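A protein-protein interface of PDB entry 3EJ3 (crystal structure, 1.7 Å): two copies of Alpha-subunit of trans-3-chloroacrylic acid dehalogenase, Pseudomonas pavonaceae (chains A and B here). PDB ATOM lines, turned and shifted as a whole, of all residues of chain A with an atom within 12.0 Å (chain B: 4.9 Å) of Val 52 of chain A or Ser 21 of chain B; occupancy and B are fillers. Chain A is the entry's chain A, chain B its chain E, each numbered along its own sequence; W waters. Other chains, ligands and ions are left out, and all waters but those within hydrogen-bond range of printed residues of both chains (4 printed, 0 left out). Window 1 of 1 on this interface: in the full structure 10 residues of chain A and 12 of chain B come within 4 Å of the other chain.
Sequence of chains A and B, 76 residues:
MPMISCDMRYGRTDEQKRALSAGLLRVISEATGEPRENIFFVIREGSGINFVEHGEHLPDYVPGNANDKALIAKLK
A ring nitrogen (NE2) of His 57 of chain A is in hydrogen-bond range of the side-chain hydroxyl of Ser 21 of chain B, at 2.7 Å. The side-chain amino group of Lys 17 of chain B is in hydrogen-bond range of the side-chain amide oxygen of Asn 50 of chain A (2.8 Å). N of Val 52 of chain A lies within hydrogen-bond range of O of Phe 41 of chain B.
O of Arg 18 of chain B lies within hydrogen-bond range of OG of Ser 21 of chain B (3.2 Å). A ring nitrogen (ND1) of His 57 of chain A lies within hydrogen-bond range of the backbone carbonyl oxygen of Ile 49 of chain A (2.7 Å). The backbone carbonyl oxygen of Leu 58 of chain A is in hydrogen-bond range of the backbone NH of Ile 49 of chain A.
Among the printed residues, merely in contact across the chains: Glu 53 of chain A with Phe 40 of chain B (3.3 Å), Val 52 of chain A with Phe 40 of chain B (3.4 Å), His 57 of chain A with Arg 18 of chain B (3.4 Å), Phe 51 of chain A with Phe 41 of chain B (3.5 Å), His 57 of chain A with Lys 17 of chain B (3.6 Å), Ile 49 of chain A with Lys 17 of chain B (3.6 Å), Asn 50 of chain A with Phe 41 of chain B (3.7 Å), Val 52 of chain A with Ser 21 of chain B (3.8 Å), Ile 49 of chain A with Arg 18 of chain B (3.8 Å) and Phe 51 of chain A with Phe 40 of chain B (3.9 Å).
Arg 44 of chain A touches none of the printed residues of chain B. Printed residues of chain B within 4 Å of Ile 49 of chain A: Lys 17 and Arg 18. Of the printed residues of chain B, Asn 50 of chain A touches Lys 17 and Phe 41. Of the printed residues of chain B, Phe 51 of chain A touches Phe 40 and Phe 41. Val 52 of chain A touches just these residues of chain B: Ser 21 (3.8 Å), Phe 40 (3.4 Å) and Phe 41 (2.8 Å). Of the printed residues of chain A, Lys 17 of chain B touches Ile 49, Asn 50 and His 57. No residue of chain A comes within 4 Å of Ala 22 of chain B. No residue of chain A comes within 4 Å of Gly 23 of chain B. No residue of chain A comes within 4 Å of Leu 24 of chain B. Of chain A, only Phe 51 (3.9 Å), Val 52 (3.4 Å) and Glu 53 (3.3 Å) come within 4 Å of Phe 40 of chain B. The nearest residue of chain B that does not touch Val 52 of chain A is Leu 25 of chain B (4.02 Å). The nearest residue of chain A that does not touch Ser 21 of chain B is Gly 55 of chain A (6.3 Å). The nearest printed residue of chain B that does not touch Ile 49 of chain A is Phe 41 of chain B (6.6 Å).
Of the 13 printed residues of chain B, 5 touch a printed residue of chain A. Of the 23 printed residues of chain A, 6 touch a printed residue of chain B. Among the printed residues, no Asp or Glu carboxylate lies within 4 Å of a Lys or Arg side-chain nitrogen of the other chain.
No position is printed for both chains. Of the 13 pairs that touch across the chains among the printed residues, none has its exchanged pair printed and touching as well.
Water W2 bridges the guanidinium group of Arg 18 of chain B (2.7 Å) and the backbone carbonyl oxygen of His 57 of chain A (3.1 Å). Water W1 bridges the guanidinium group of Arg 18 of chain B and the backbone NH of His 57 of chain A.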
ATOM      1  N   ASP A   7      22.601 -13.060 -17.934  1.00  0.00           N
ATOM      2  CA  ASP A   7      22.044 -11.694 -18.167  1.00  0.00           C
ATOM      3  C   ASP A   7      22.670 -11.097 -19.425  1.00  0.00           C
ATOM      4  O   ASP A   7      23.909 -10.977 -19.514  1.00  0.00           O
ATOM      5  CB  ASP A   7      22.354 -10.738 -17.026  1.00  0.00           C
ATOM      6  CG  ASP A   7      21.526 -11.010 -15.777  1.00  0.00           C
ATOM      7  OD1 ASP A   7      20.521 -10.318 -15.582  1.00  0.00           O
ATOM      8  OD2 ASP A   7      21.903 -11.874 -14.949  1.00  0.00           O
ATOM      9  N   MET A   8      21.833 -10.670 -20.374  1.00  0.00           N
ATOM     10  CA  MET A   8      22.355 -10.045 -21.603  1.00  0.00           C
ATOM     11  C   MET A   8      21.297  -9.172 -22.258  1.00  0.00           C
ATOM     12  O   MET A   8      20.137  -9.215 -21.877  1.00  0.00           O
ATOM     13  CB  MET A   8      22.856 -11.122 -22.580  1.00  0.00           C
ATOM     14  CG  MET A   8      21.762 -11.961 -23.197  1.00  0.00           C
ATOM     15  SD  MET A   8      22.539 -13.188 -24.301  1.00  0.00           S
ATOM     16  CE  MET A   8      21.138 -14.193 -24.716  1.00  0.00           C
ATOM     17  N   ARG A   9      21.698  -8.388 -23.242  1.00  0.00           N
ATOM     18  CA  ARG A   9      20.760  -7.477 -23.884  1.00  0.00           C
ATOM     19  C   ARG A   9      19.785  -8.266 -24.733  1.00  0.00           C
ATOM     20  O   ARG A   9      20.161  -9.300 -25.298  1.00  0.00           O
ATOM     21  CB  ARG A   9      21.542  -6.520 -24.788  1.00  0.00           C
ATOM     22  CG  ARG A   9      22.279  -5.449 -24.004  1.00  0.00           C
ATOM     23  CD  ARG A   9      23.215  -4.670 -24.935  1.00  0.00           C
ATOM     24  NE  ARG A   9      24.300  -5.524 -25.440  1.00  0.00           N
ATOM     25  CZ  ARG A   9      25.134  -5.159 -26.425  1.00  0.00           C
ATOM     26  NH1 ARG A   9      24.975  -3.996 -27.043  1.00  0.00           N
ATOM     27  NH2 ARG A   9      26.092  -5.969 -26.814  1.00  0.00           N
ATOM     28  N   TYR A  10      18.560  -7.755 -24.861  1.00  0.00           N
ATOM     29  CA  TYR A  10      17.608  -8.193 -25.912  1.00  0.00           C
ATOM     30  C   TYR A  10      18.288  -8.249 -27.263  1.00  0.00           C
ATOM     31  O   TYR A  10      19.170  -7.431 -27.555  1.00  0.00           O
ATOM     32  CB  TYR A  10      16.416  -7.200 -26.074  1.00  0.00           C
ATOM     33  CG  TYR A  10      15.510  -7.180 -24.878  1.00  0.00           C
ATOM     34  CD1 TYR A  10      14.661  -8.259 -24.612  1.00  0.00           C
ATOM     35  CD2 TYR A  10      15.500  -6.086 -23.992  1.00  0.00           C
ATOM     36  CE1 TYR A  10      13.836  -8.272 -23.493  1.00  0.00           C
ATOM     37  CE2 TYR A  10      14.670  -6.072 -22.872  1.00  0.00           C
ATOM     38  CZ  TYR A  10      13.843  -7.174 -22.621  1.00  0.00           C
ATOM     39  OH  TYR A  10      13.032  -7.193 -21.503  1.00  0.00           O
ATOM     40  N   ARG A  12      19.128 -11.368 -29.189  1.00  0.00           N
ATOM     41  CA  ARG A  12      19.621 -12.654 -29.717  1.00  0.00           C
ATOM     42  C   ARG A  12      18.436 -13.459 -30.237  1.00  0.00           C
ATOM     43  O   ARG A  12      17.344 -13.434 -29.661  1.00  0.00           O
ATOM     44  CB  ARG A  12      20.397 -13.460 -28.661  1.00  0.00           C
ATOM     45  CG  ARG A  12      21.868 -13.033 -28.463  1.00  0.00           C
ATOM     46  CD  ARG A  12      22.022 -11.667 -27.796  1.00  0.00           C
ATOM     47  NE  ARG A  12      23.434 -11.299 -27.647  1.00  0.00           N
ATOM     48  CZ  ARG A  12      23.914 -10.402 -26.780  1.00  0.00           C
ATOM     49  NH1 ARG A  12      25.232 -10.171 -26.722  1.00  0.00           N
ATOM     50  NH2 ARG A  12      23.098  -9.715 -25.980  1.00  0.00           N
ATOM     51  N   ARG A  44      18.118 -13.750 -18.803  1.00  0.00           N
ATOM     52  CA  ARG A  44      17.440 -12.523 -18.314  1.00  0.00           C
ATOM     53  C   ARG A  44      17.896 -11.383 -19.221  1.00  0.00           C
ATOM     54  O   ARG A  44      19.080 -11.054 -19.270  1.00  0.00           O
ATOM     55  CB  ARG A  44      17.821 -12.210 -16.875  1.00  0.00           C
ATOM     56  CG  ARG A  44      17.557 -13.340 -15.887  1.00  0.00           C
ATOM     57  CD  ARG A  44      18.020 -12.884 -14.499  1.00  0.00           C
ATOM     58  NE  ARG A  44      17.791 -13.927 -13.488  1.00  0.00           N
ATOM     59  CZ  ARG A  44      18.741 -14.386 -12.687  1.00  0.00           C
ATOM     60  NH1 ARG A  44      19.970 -13.895 -12.777  1.00  0.00           N
ATOM     61  NH2 ARG A  44      18.460 -15.306 -11.794  1.00  0.00           N
ATOM     62  N   GLU A  45      16.947 -10.813 -19.959  1.00  0.00           N
ATOM     63  CA  GLU A  45      17.238  -9.807 -20.981  1.00  0.00           C
ATOM     64  C   GLU A  45      16.912  -8.412 -20.482  1.00  0.00           C
ATOM     65  O   GLU A  45      15.995  -8.239 -19.679  1.00  0.00           O
ATOM     66  CB  GLU A  45      16.391 -10.087 -22.236  1.00  0.00           C
ATOM     67  CG  GLU A  45      16.793 -11.336 -22.968  1.00  0.00           C
ATOM     68  CD  GLU A  45      15.870 -11.612 -24.137  1.00  0.00           C
ATOM     69  OE1 GLU A  45      14.674 -11.815 -23.876  1.00  0.00           O
ATOM     70  OE2 GLU A  45      16.353 -11.629 -25.296  1.00  0.00           O
ATOM     71  N   GLY A  46      17.651  -7.417 -20.968  1.00  0.00           N
ATOM     72  CA  GLY A  46      17.354  -6.014 -20.643  1.00  0.00           C
ATOM     73  C   GLY A  46      17.837  -5.096 -21.762  1.00  0.00           C
ATOM     74  O   GLY A  46      18.555  -5.539 -22.661  1.00  0.00           O
ATOM     75  N   SER A  47      17.420  -3.830 -21.679  1.00  0.00           N
ATOM     76  CA  SER A  47      17.878  -2.767 -22.582  1.00  0.00           C
ATOM     77  C   SER A  47      19.383  -2.553 -22.470  1.00  0.00           C
ATOM     78  O   SER A  47      20.005  -2.916 -21.466  1.00  0.00           O
ATOM     79  CB  SER A  47      17.163  -1.434 -22.273  1.00  0.00           C
ATOM     80  OG  SER A  47      15.760  -1.586 -22.232  1.00  0.00           O
ATOM     81  N   GLY A  48      19.969  -1.953 -23.502  1.00  0.00           N
ATOM     82  CA  GLY A  48      21.403  -1.663 -23.491  1.00  0.00           C
ATOM     83  C   GLY A  48      21.890  -0.814 -22.340  1.00  0.00           C
ATOM     84  O   GLY A  48      22.938  -1.130 -21.741  1.00  0.00           O
ATOM     85  N   ILE A  49      21.125   0.233 -22.001  1.00  0.00           N
ATOM     86  CA  ILE A  49      21.469   1.171 -20.915  1.00  0.00           C
ATOM     87  C   ILE A  49      21.617   0.440 -19.576  1.00  0.00           C
ATOM     88  O   ILE A  49      22.307   0.895 -18.677  1.00  0.00           O
ATOM     89  CB  ILE A  49      20.403   2.324 -20.799  1.00  0.00           C
ATOM     90  CG1 ILE A  49      20.853   3.453 -19.853  1.00  0.00           C
ATOM     91  CG2 ILE A  49      19.026   1.777 -20.404  1.00  0.00           C
ATOM     92  CD1 ILE A  49      21.970   4.291 -20.391  1.00  0.00           C
ATOM     93  N   ASN A  50      20.986  -0.718 -19.470  1.00  0.00           N
ATOM     94  CA  ASN A  50      21.041  -1.475 -18.237  1.00  0.00           C
ATOM     95  C   ASN A  50      22.343  -2.262 -18.000  1.00  0.00           C
ATOM     96  O   ASN A  50      22.493  -2.857 -16.926  1.00  0.00           O
ATOM     97  CB  ASN A  50      19.870  -2.457 -18.211  1.00  0.00           C
ATOM     98  CG  ASN A  50      18.547  -1.789 -17.974  1.00  0.00           C
ATOM     99  OD1 ASN A  50      18.447  -0.572 -17.772  1.00  0.00           O
ATOM    100  ND2 ASN A  50      17.481  -2.610 -17.982  1.00  0.00           N
ATOM    101  N   PHE A  51      23.242  -2.277 -18.979  1.00  0.00           N
ATOM    102  CA  PHE A  51      24.494  -3.043 -18.915  1.00  0.00           C
ATOM    103  C   PHE A  51      25.691  -2.114 -18.942  1.00  0.00           C
ATOM    104  O   PHE A  51      25.778  -1.273 -19.839  1.00  0.00           O
ATOM    105  CB  PHE A  51      24.553  -3.994 -20.094  1.00  0.00           C
ATOM    106  CG  PHE A  51      23.559  -5.116 -19.982  1.00  0.00           C
ATOM    107  CD1 PHE A  51      22.251  -4.936 -20.394  1.00  0.00           C
ATOM    108  CD2 PHE A  51      23.914  -6.312 -19.384  1.00  0.00           C
ATOM    109  CE1 PHE A  51      21.301  -5.946 -20.243  1.00  0.00           C
ATOM    110  CE2 PHE A  51      22.974  -7.337 -19.217  1.00  0.00           C
ATOM    111  CZ  PHE A  51      21.681  -7.162 -19.675  1.00  0.00           C
ATOM    112  N   VAL A  52      26.589  -2.267 -17.971  1.00  0.00           N
ATOM    113  CA  VAL A  52      27.857  -1.508 -17.944  1.00  0.00           C
ATOM    114  C   VAL A  52      28.998  -2.526 -18.017  1.00  0.00           C
ATOM    115  O   VAL A  52      29.191  -3.332 -17.093  1.00  0.00           O
ATOM    116  CB  VAL A  52      27.966  -0.628 -16.681  1.00  0.00           C
ATOM    117  CG1 VAL A  52      29.205   0.250 -16.736  1.00  0.00           C
ATOM    118  CG2 VAL A  52      26.746   0.243 -16.545  1.00  0.00           C
ATOM    119  N   GLU A  53      29.749  -2.456 -19.125  1.00  0.00           N
ATOM    120  CA  GLU A  53      30.781  -3.409 -19.493  1.00  0.00           C
ATOM    121  C   GLU A  53      32.064  -2.610 -19.809  1.00  0.00           C
ATOM    122  O   GLU A  53      32.025  -1.656 -20.612  1.00  0.00           O
ATOM    123  CB  GLU A  53      30.321  -4.150 -20.752  1.00  0.00           C
ATOM    124  CG  GLU A  53      31.218  -5.259 -21.233  1.00  0.00           C
ATOM    125  CD  GLU A  53      31.338  -6.391 -20.214  1.00  0.00           C
ATOM    126  OE1 GLU A  53      30.298  -6.982 -19.838  1.00  0.00           O
ATOM    127  OE2 GLU A  53      32.479  -6.703 -19.815  1.00  0.00           O
ATOM    128  N   HIS A  54      33.182  -2.979 -19.191  1.00  0.00           N
ATOM    129  CA  HIS A  54      34.424  -2.184 -19.346  1.00  0.00           C
ATOM    130  C   HIS A  54      34.168  -0.722 -19.024  1.00  0.00           C
ATOM    131  O   HIS A  54      34.692   0.185 -19.685  1.00  0.00           O
ATOM    132  CB  HIS A  54      34.980  -2.310 -20.752  1.00  0.00           C
ATOM    133  CG  HIS A  54      35.483  -3.671 -21.071  1.00  0.00           C
ATOM    134  ND1 HIS A  54      36.758  -4.083 -20.748  1.00  0.00           N
ATOM    135  CD2 HIS A  54      34.885  -4.720 -21.681  1.00  0.00           C
ATOM    136  CE1 HIS A  54      36.924  -5.331 -21.148  1.00  0.00           C
ATOM    137  NE2 HIS A  54      35.801  -5.741 -21.713  1.00  0.00           N
ATOM    138  N   GLY A  55      33.347  -0.494 -18.009  1.00  0.00           N
ATOM    139  CA  GLY A  55      33.033   0.850 -17.533  1.00  0.00           C
ATOM    140  C   GLY A  55      32.142   1.742 -18.387  1.00  0.00           C
ATOM    141  O   GLY A  55      32.030   2.935 -18.117  1.00  0.00           O
ATOM    142  N   GLU A  56      31.490   1.201 -19.410  1.00  0.00           N
ATOM    143  CA  GLU A  56      30.590   2.035 -20.209  1.00  0.00           C
ATOM    144  C   GLU A  56      29.256   1.341 -20.465  1.00  0.00           C
ATOM    145  O   GLU A  56      29.215   0.116 -20.646  1.00  0.00           O
ATOM    146  CB  GLU A  56      31.266   2.531 -21.499  1.00  0.00           C
ATOM    147  CG  GLU A  56      32.326   3.678 -21.240  1.00  0.00           C
ATOM    148  CD  GLU A  56      32.723   4.514 -22.475  1.00  0.00           C
ATOM    149  OE1 GLU A  56      31.968   4.556 -23.489  1.00  0.00           O
ATOM    150  OE2 GLU A  56      33.808   5.165 -22.418  1.00  0.00           O
ATOM    151  N   HIS A  57      28.190   2.136 -20.433  1.00  0.00           N
ATOM    152  CA  HIS A  57      26.824   1.653 -20.673  1.00  0.00           C
ATOM    153  C   HIS A  57      26.746   1.255 -22.140  1.00  0.00           C
ATOM    154  O   HIS A  57      27.292   1.951 -23.025  1.00  0.00           O
ATOM    155  CB  HIS A  57      25.797   2.743 -20.362  1.00  0.00           C
ATOM    156  CG  HIS A  57      25.577   2.983 -18.902  1.00  0.00           C
ATOM    157  ND1 HIS A  57      24.474   2.504 -18.232  1.00  0.00           N
ATOM    158  CD2 HIS A  57      26.315   3.655 -17.981  1.00  0.00           C
ATOM    159  CE1 HIS A  57      24.543   2.865 -16.958  1.00  0.00           C
ATOM    160  NE2 HIS A  57      25.649   3.567 -16.784  1.00  0.00           N
ATOM    161  N   LEU A  58      26.092   0.126 -22.398  1.00  0.00           N
ATOM    162  CA  LEU A  58      26.005  -0.426 -23.745  1.00  0.00           C
ATOM    163  C   LEU A  58      24.851   0.167 -24.538  1.00  0.00           C
ATOM    164  O   LEU A  58      23.834   0.576 -23.969  1.00  0.00           O
ATOM    165  CB  LEU A  58      25.875  -1.946 -23.705  1.00  0.00           C
ATOM    166  CG  LEU A  58      26.993  -2.769 -23.069  1.00  0.00           C
ATOM    167  CD1 LEU A  58      26.674  -4.246 -23.226  1.00  0.00           C
ATOM    168  CD2 LEU A  58      28.338  -2.469 -23.694  1.00  0.00           C
ATOM    169  N   PRO A  59      25.003   0.221 -25.875  1.00  0.00           N
ATOM    170  CA  PRO A  59      23.890   0.606 -26.719  1.00  0.00           C
ATOM    171  C   PRO A  59      22.928  -0.572 -26.823  1.00  0.00           C
ATOM    172  O   PRO A  59      23.328  -1.707 -26.522  1.00  0.00           O
ATOM    173  CB  PRO A  59      24.554   0.842 -28.073  1.00  0.00           C
ATOM    174  CG  PRO A  59      25.706  -0.010 -28.104  1.00  0.00           C
ATOM    175  CD  PRO A  59      26.215  -0.076 -26.658  1.00  0.00           C
ATOM    176  N   ASP A  60      21.685  -0.305 -27.231  1.00  0.00           N
ATOM    177  CA  ASP A  60      20.771  -1.395 -27.581  1.00  0.00           C
ATOM    178  C   ASP A  60      21.397  -2.232 -28.698  1.00  0.00           C
ATOM    179  O   ASP A  60      21.952  -1.685 -29.677  1.00  0.00           O
ATOM    180  CB  ASP A  60      19.366  -0.862 -27.929  1.00  0.00           C
ATOM    181  CG  ASP A  60      18.564  -0.444 -26.674  1.00  0.00           C
ATOM    182  OD1 ASP A  60      18.178   0.746 -26.558  1.00  0.00           O
ATOM    183  OD2 ASP A  60      18.286  -1.307 -25.797  1.00  0.00           O
ATOM    184  N   TYR A  61      21.322  -3.555 -28.533  1.00  0.00           N
ATOM    185  CA  TYR A  61      21.951  -4.537 -29.403  1.00  0.00           C
ATOM    186  C   TYR A  61      21.311  -4.536 -30.784  1.00  0.00           C
ATOM    187  O   TYR A  61      20.079  -4.506 -30.940  1.00  0.00           O
ATOM    188  CB  TYR A  61      21.866  -5.930 -28.752  1.00  0.00           C
ATOM    189  CG  TYR A  61      22.484  -7.087 -29.502  1.00  0.00           C
ATOM    190  CD1 TYR A  61      23.827  -7.409 -29.351  1.00  0.00           C
ATOM    191  CD2 TYR A  61      21.704  -7.902 -30.327  1.00  0.00           C
ATOM    192  CE1 TYR A  61      24.391  -8.502 -30.034  1.00  0.00           C
ATOM    193  CE2 TYR A  61      22.252  -8.985 -31.006  1.00  0.00           C
ATOM    194  CZ  TYR A  61      23.588  -9.281 -30.855  1.00  0.00           C
ATOM    195  OH  TYR A  61      24.120 -10.358 -31.535  1.00  0.00           O
ATOM    196  N   LYS B  17      20.285   6.271 -14.538  1.00  0.00           N
ATOM    197  CA  LYS B  17      20.998   4.959 -14.586  1.00  0.00           C
ATOM    198  C   LYS B  17      22.519   5.185 -14.667  1.00  0.00           C
ATOM    199  O   LYS B  17      23.312   4.468 -14.019  1.00  0.00           O
ATOM    200  CB  LYS B  17      20.491   4.079 -15.730  1.00  0.00           C
ATOM    201  CG  LYS B  17      19.035   3.693 -15.583  1.00  0.00           C
ATOM    202  CD  LYS B  17      18.653   2.680 -16.660  1.00  0.00           C
ATOM    203  CE  LYS B  17      17.266   2.102 -16.386  1.00  0.00           C
ATOM    204  NZ  LYS B  17      16.687   1.581 -17.660  1.00  0.00           N
ATOM    205  N   ARG B  18      22.936   6.208 -15.424  1.00  0.00           N
ATOM    206  CA  ARG B  18      24.371   6.514 -15.537  1.00  0.00           C
ATOM    207  C   ARG B  18      24.904   7.078 -14.218  1.00  0.00           C
ATOM    208  O   ARG B  18      26.056   6.816 -13.848  1.00  0.00           O
ATOM    209  CB  ARG B  18      24.647   7.462 -16.721  1.00  0.00           C
ATOM    210  CG  ARG B  18      24.447   6.812 -18.111  1.00  0.00           C
ATOM    211  CD  ARG B  18      24.920   7.749 -19.237  1.00  0.00           C
ATOM    212  NE  ARG B  18      24.349   7.410 -20.543  1.00  0.00           N
ATOM    213  CZ  ARG B  18      24.929   6.617 -21.439  1.00  0.00           C
ATOM    214  NH1 ARG B  18      24.328   6.373 -22.594  1.00  0.00           N
ATOM    215  NH2 ARG B  18      26.107   6.071 -21.189  1.00  0.00           N
ATOM    216  N   ALA B  19      24.070   7.838 -13.505  1.00  0.00           N
ATOM    217  CA  ALA B  19      24.455   8.337 -12.187  1.00  0.00           C
ATOM    218  C   ALA B  19      24.584   7.194 -11.197  1.00  0.00           C
ATOM    219  O   ALA B  19      25.517   7.157 -10.365  1.00  0.00           O
ATOM    220  CB  ALA B  19      23.484   9.421 -11.700  1.00  0.00           C
ATOM    221  N   LEU B  20      23.673   6.226 -11.316  1.00  0.00           N
ATOM    222  CA  LEU B  20      23.695   5.085 -10.434  1.00  0.00           C
ATOM    223  C   LEU B  20      24.962   4.255 -10.656  1.00  0.00           C
ATOM    224  O   LEU B  20      25.661   3.888  -9.700  1.00  0.00           O
ATOM    225  CB  LEU B  20      22.439   4.227 -10.671  1.00  0.00           C
ATOM    226  CG  LEU B  20      22.338   2.943  -9.835  1.00  0.00           C
ATOM    227  CD1 LEU B  20      22.350   3.165  -8.334  1.00  0.00           C
ATOM    228  CD2 LEU B  20      21.103   2.190 -10.314  1.00  0.00           C
ATOM    229  N   SER B  21      25.265   3.956 -11.918  1.00  0.00           N
ATOM    230  CA  SER B  21      26.424   3.108 -12.209  1.00  0.00           C
ATOM    231  C   SER B  21      27.708   3.842 -11.799  1.00  0.00           C
ATOM    232  O   SER B  21      28.606   3.224 -11.236  1.00  0.00           O
ATOM    233  CB  SER B  21      26.493   2.719 -13.677  1.00  0.00           C
ATOM    234  OG  SER B  21      26.956   3.825 -14.464  1.00  0.00           O
ATOM    235  N   ALA B  22      27.795   5.150 -12.077  1.00  0.00           N
ATOM    236  CA  ALA B  22      28.984   5.924 -11.650  1.00  0.00           C
ATOM    237  C   ALA B  22      29.246   5.782 -10.139  1.00  0.00           C
ATOM    238  O   ALA B  22      30.398   5.528  -9.723  1.00  0.00           O
ATOM    239  CB  ALA B  22      28.838   7.410 -12.032  1.00  0.00           C
ATOM    240  N   GLY B  23      28.186   5.933  -9.343  1.00  0.00           N
ATOM    241  CA  GLY B  23      28.252   5.871  -7.856  1.00  0.00           C
ATOM    242  C   GLY B  23      28.653   4.474  -7.424  1.00  0.00           C
ATOM    243  O   GLY B  23      29.601   4.303  -6.616  1.00  0.00           O
ATOM    244  N   LEU B  24      27.930   3.470  -7.932  1.00  0.00           N
ATOM    245  CA  LEU B  24      28.232   2.060  -7.562  1.00  0.00           C
ATOM    246  C   LEU B  24      29.647   1.604  -7.960  1.00  0.00           C
ATOM    247  O   LEU B  24      30.379   1.029  -7.130  1.00  0.00           O
ATOM    248  CB  LEU B  24      27.150   1.120  -8.109  1.00  0.00           C
ATOM    249  CG  LEU B  24      25.788   1.320  -7.468  1.00  0.00           C
ATOM    250  CD1 LEU B  24      24.809   0.367  -8.204  1.00  0.00           C
ATOM    251  CD2 LEU B  24      25.749   1.034  -5.957  1.00  0.00           C
ATOM    252  N   LEU B  25      30.076   1.949  -9.182  1.00  0.00           N
ATOM    253  CA  LEU B  25      31.442   1.605  -9.622  1.00  0.00           C
ATOM    254  C   LEU B  25      32.497   2.296  -8.730  1.00  0.00           C
ATOM    255  O   LEU B  25      33.481   1.685  -8.345  1.00  0.00           O
ATOM    256  CB  LEU B  25      31.634   1.941 -11.112  1.00  0.00           C
ATOM    257  CG  LEU B  25      31.247   0.809 -12.075  1.00  0.00           C
ATOM    258  CD1 LEU B  25      29.866   0.174 -11.852  1.00  0.00           C
ATOM    259  CD2 LEU B  25      31.322   1.349 -13.498  1.00  0.00           C
ATOM    260  N   ARG B  26      32.245   3.549  -8.355  1.00  0.00           N
ATOM    261  CA  ARG B  26      33.190   4.267  -7.476  1.00  0.00           C
ATOM    262  C   ARG B  26      33.294   3.534  -6.144  1.00  0.00           C
ATOM    263  O   ARG B  26      34.397   3.284  -5.645  1.00  0.00           O
ATOM    264  CB  ARG B  26      32.697   5.700  -7.255  1.00  0.00           C
ATOM    265  CG  ARG B  26      33.683   6.655  -6.591  1.00  0.00           C
ATOM    266  CD  ARG B  26      32.873   7.758  -5.928  1.00  0.00           C
ATOM    267  NE  ARG B  26      32.725   7.319  -4.572  1.00  0.00           N
ATOM    268  CZ  ARG B  26      31.752   7.595  -3.729  1.00  0.00           C
ATOM    269  NH1 ARG B  26      30.687   8.341  -4.040  1.00  0.00           N
ATOM    270  NH2 ARG B  26      31.872   7.067  -2.526  1.00  0.00           N
ATOM    271  N   ILE B  39      34.421  -4.073 -13.391  1.00  0.00           N
ATOM    272  CA  ILE B  39      33.392  -3.954 -12.359  1.00  0.00           C
ATOM    273  C   ILE B  39      32.149  -3.998 -13.279  1.00  0.00           C
ATOM    274  O   ILE B  39      31.690  -2.941 -13.796  1.00  0.00           O
ATOM    275  CB  ILE B  39      33.313  -2.684 -11.525  1.00  0.00           C
ATOM    276  CG1 ILE B  39      34.487  -2.627 -10.553  1.00  0.00           C
ATOM    277  CG2 ILE B  39      31.991  -2.729 -10.716  1.00  0.00           C
ATOM    278  CD1 ILE B  39      34.552  -1.329  -9.747  1.00  0.00           C
ATOM    279  N   PHE B  40      31.616  -5.186 -13.518  1.00  0.00           N
ATOM    280  CA  PHE B  40      30.453  -5.315 -14.419  1.00  0.00           C
ATOM    281  C   PHE B  40      29.181  -4.952 -13.652  1.00  0.00           C
ATOM    282  O   PHE B  40      29.058  -5.299 -12.487  1.00  0.00           O
ATOM    283  CB  PHE B  40      30.371  -6.741 -14.958  1.00  0.00           C
ATOM    284  CG  PHE B  40      29.053  -7.080 -15.616  1.00  0.00           C
ATOM    285  CD1 PHE B  40      28.815  -6.727 -16.936  1.00  0.00           C
ATOM    286  CD2 PHE B  40      28.038  -7.695 -14.906  1.00  0.00           C
ATOM    287  CE1 PHE B  40      27.585  -7.038 -17.575  1.00  0.00           C
ATOM    288  CE2 PHE B  40      26.807  -7.998 -15.519  1.00  0.00           C
ATOM    289  CZ  PHE B  40      26.588  -7.666 -16.854  1.00  0.00           C
ATOM    290  N   PHE B  41      28.232  -4.289 -14.318  1.00  0.00           N
ATOM    291  CA  PHE B  41      26.987  -3.904 -13.666  1.00  0.00           C
ATOM    292  C   PHE B  41      25.810  -4.187 -14.558  1.00  0.00           C
ATOM    293  O   PHE B  41      25.820  -3.834 -15.744  1.00  0.00           O
ATOM    294  CB  PHE B  41      27.037  -2.421 -13.297  1.00  0.00           C
ATOM    295  CG  PHE B  41      25.784  -1.872 -12.646  1.00  0.00           C
ATOM    296  CD1 PHE B  41      25.086  -2.569 -11.628  1.00  0.00           C
ATOM    297  CD2 PHE B  41      25.352  -0.607 -12.993  1.00  0.00           C
ATOM    298  CE1 PHE B  41      23.934  -1.964 -10.999  1.00  0.00           C
ATOM    299  CE2 PHE B  41      24.228  -0.015 -12.405  1.00  0.00           C
ATOM    300  CZ  PHE B  41      23.511  -0.703 -11.406  1.00  0.00           C
HETATM  301  O   HOH W   1      28.803   5.133 -20.152  1.00  0.00           O
HETATM  302  O   HOH W   2      25.554   4.357 -23.931  1.00  0.00           O
HETATM  303  O   HOH W   3      32.027  -2.259 -16.377  1.00  0.00           O
HETATM  304  O   HOH W   4      14.721   0.179 -20.092  1.00  0.00           O
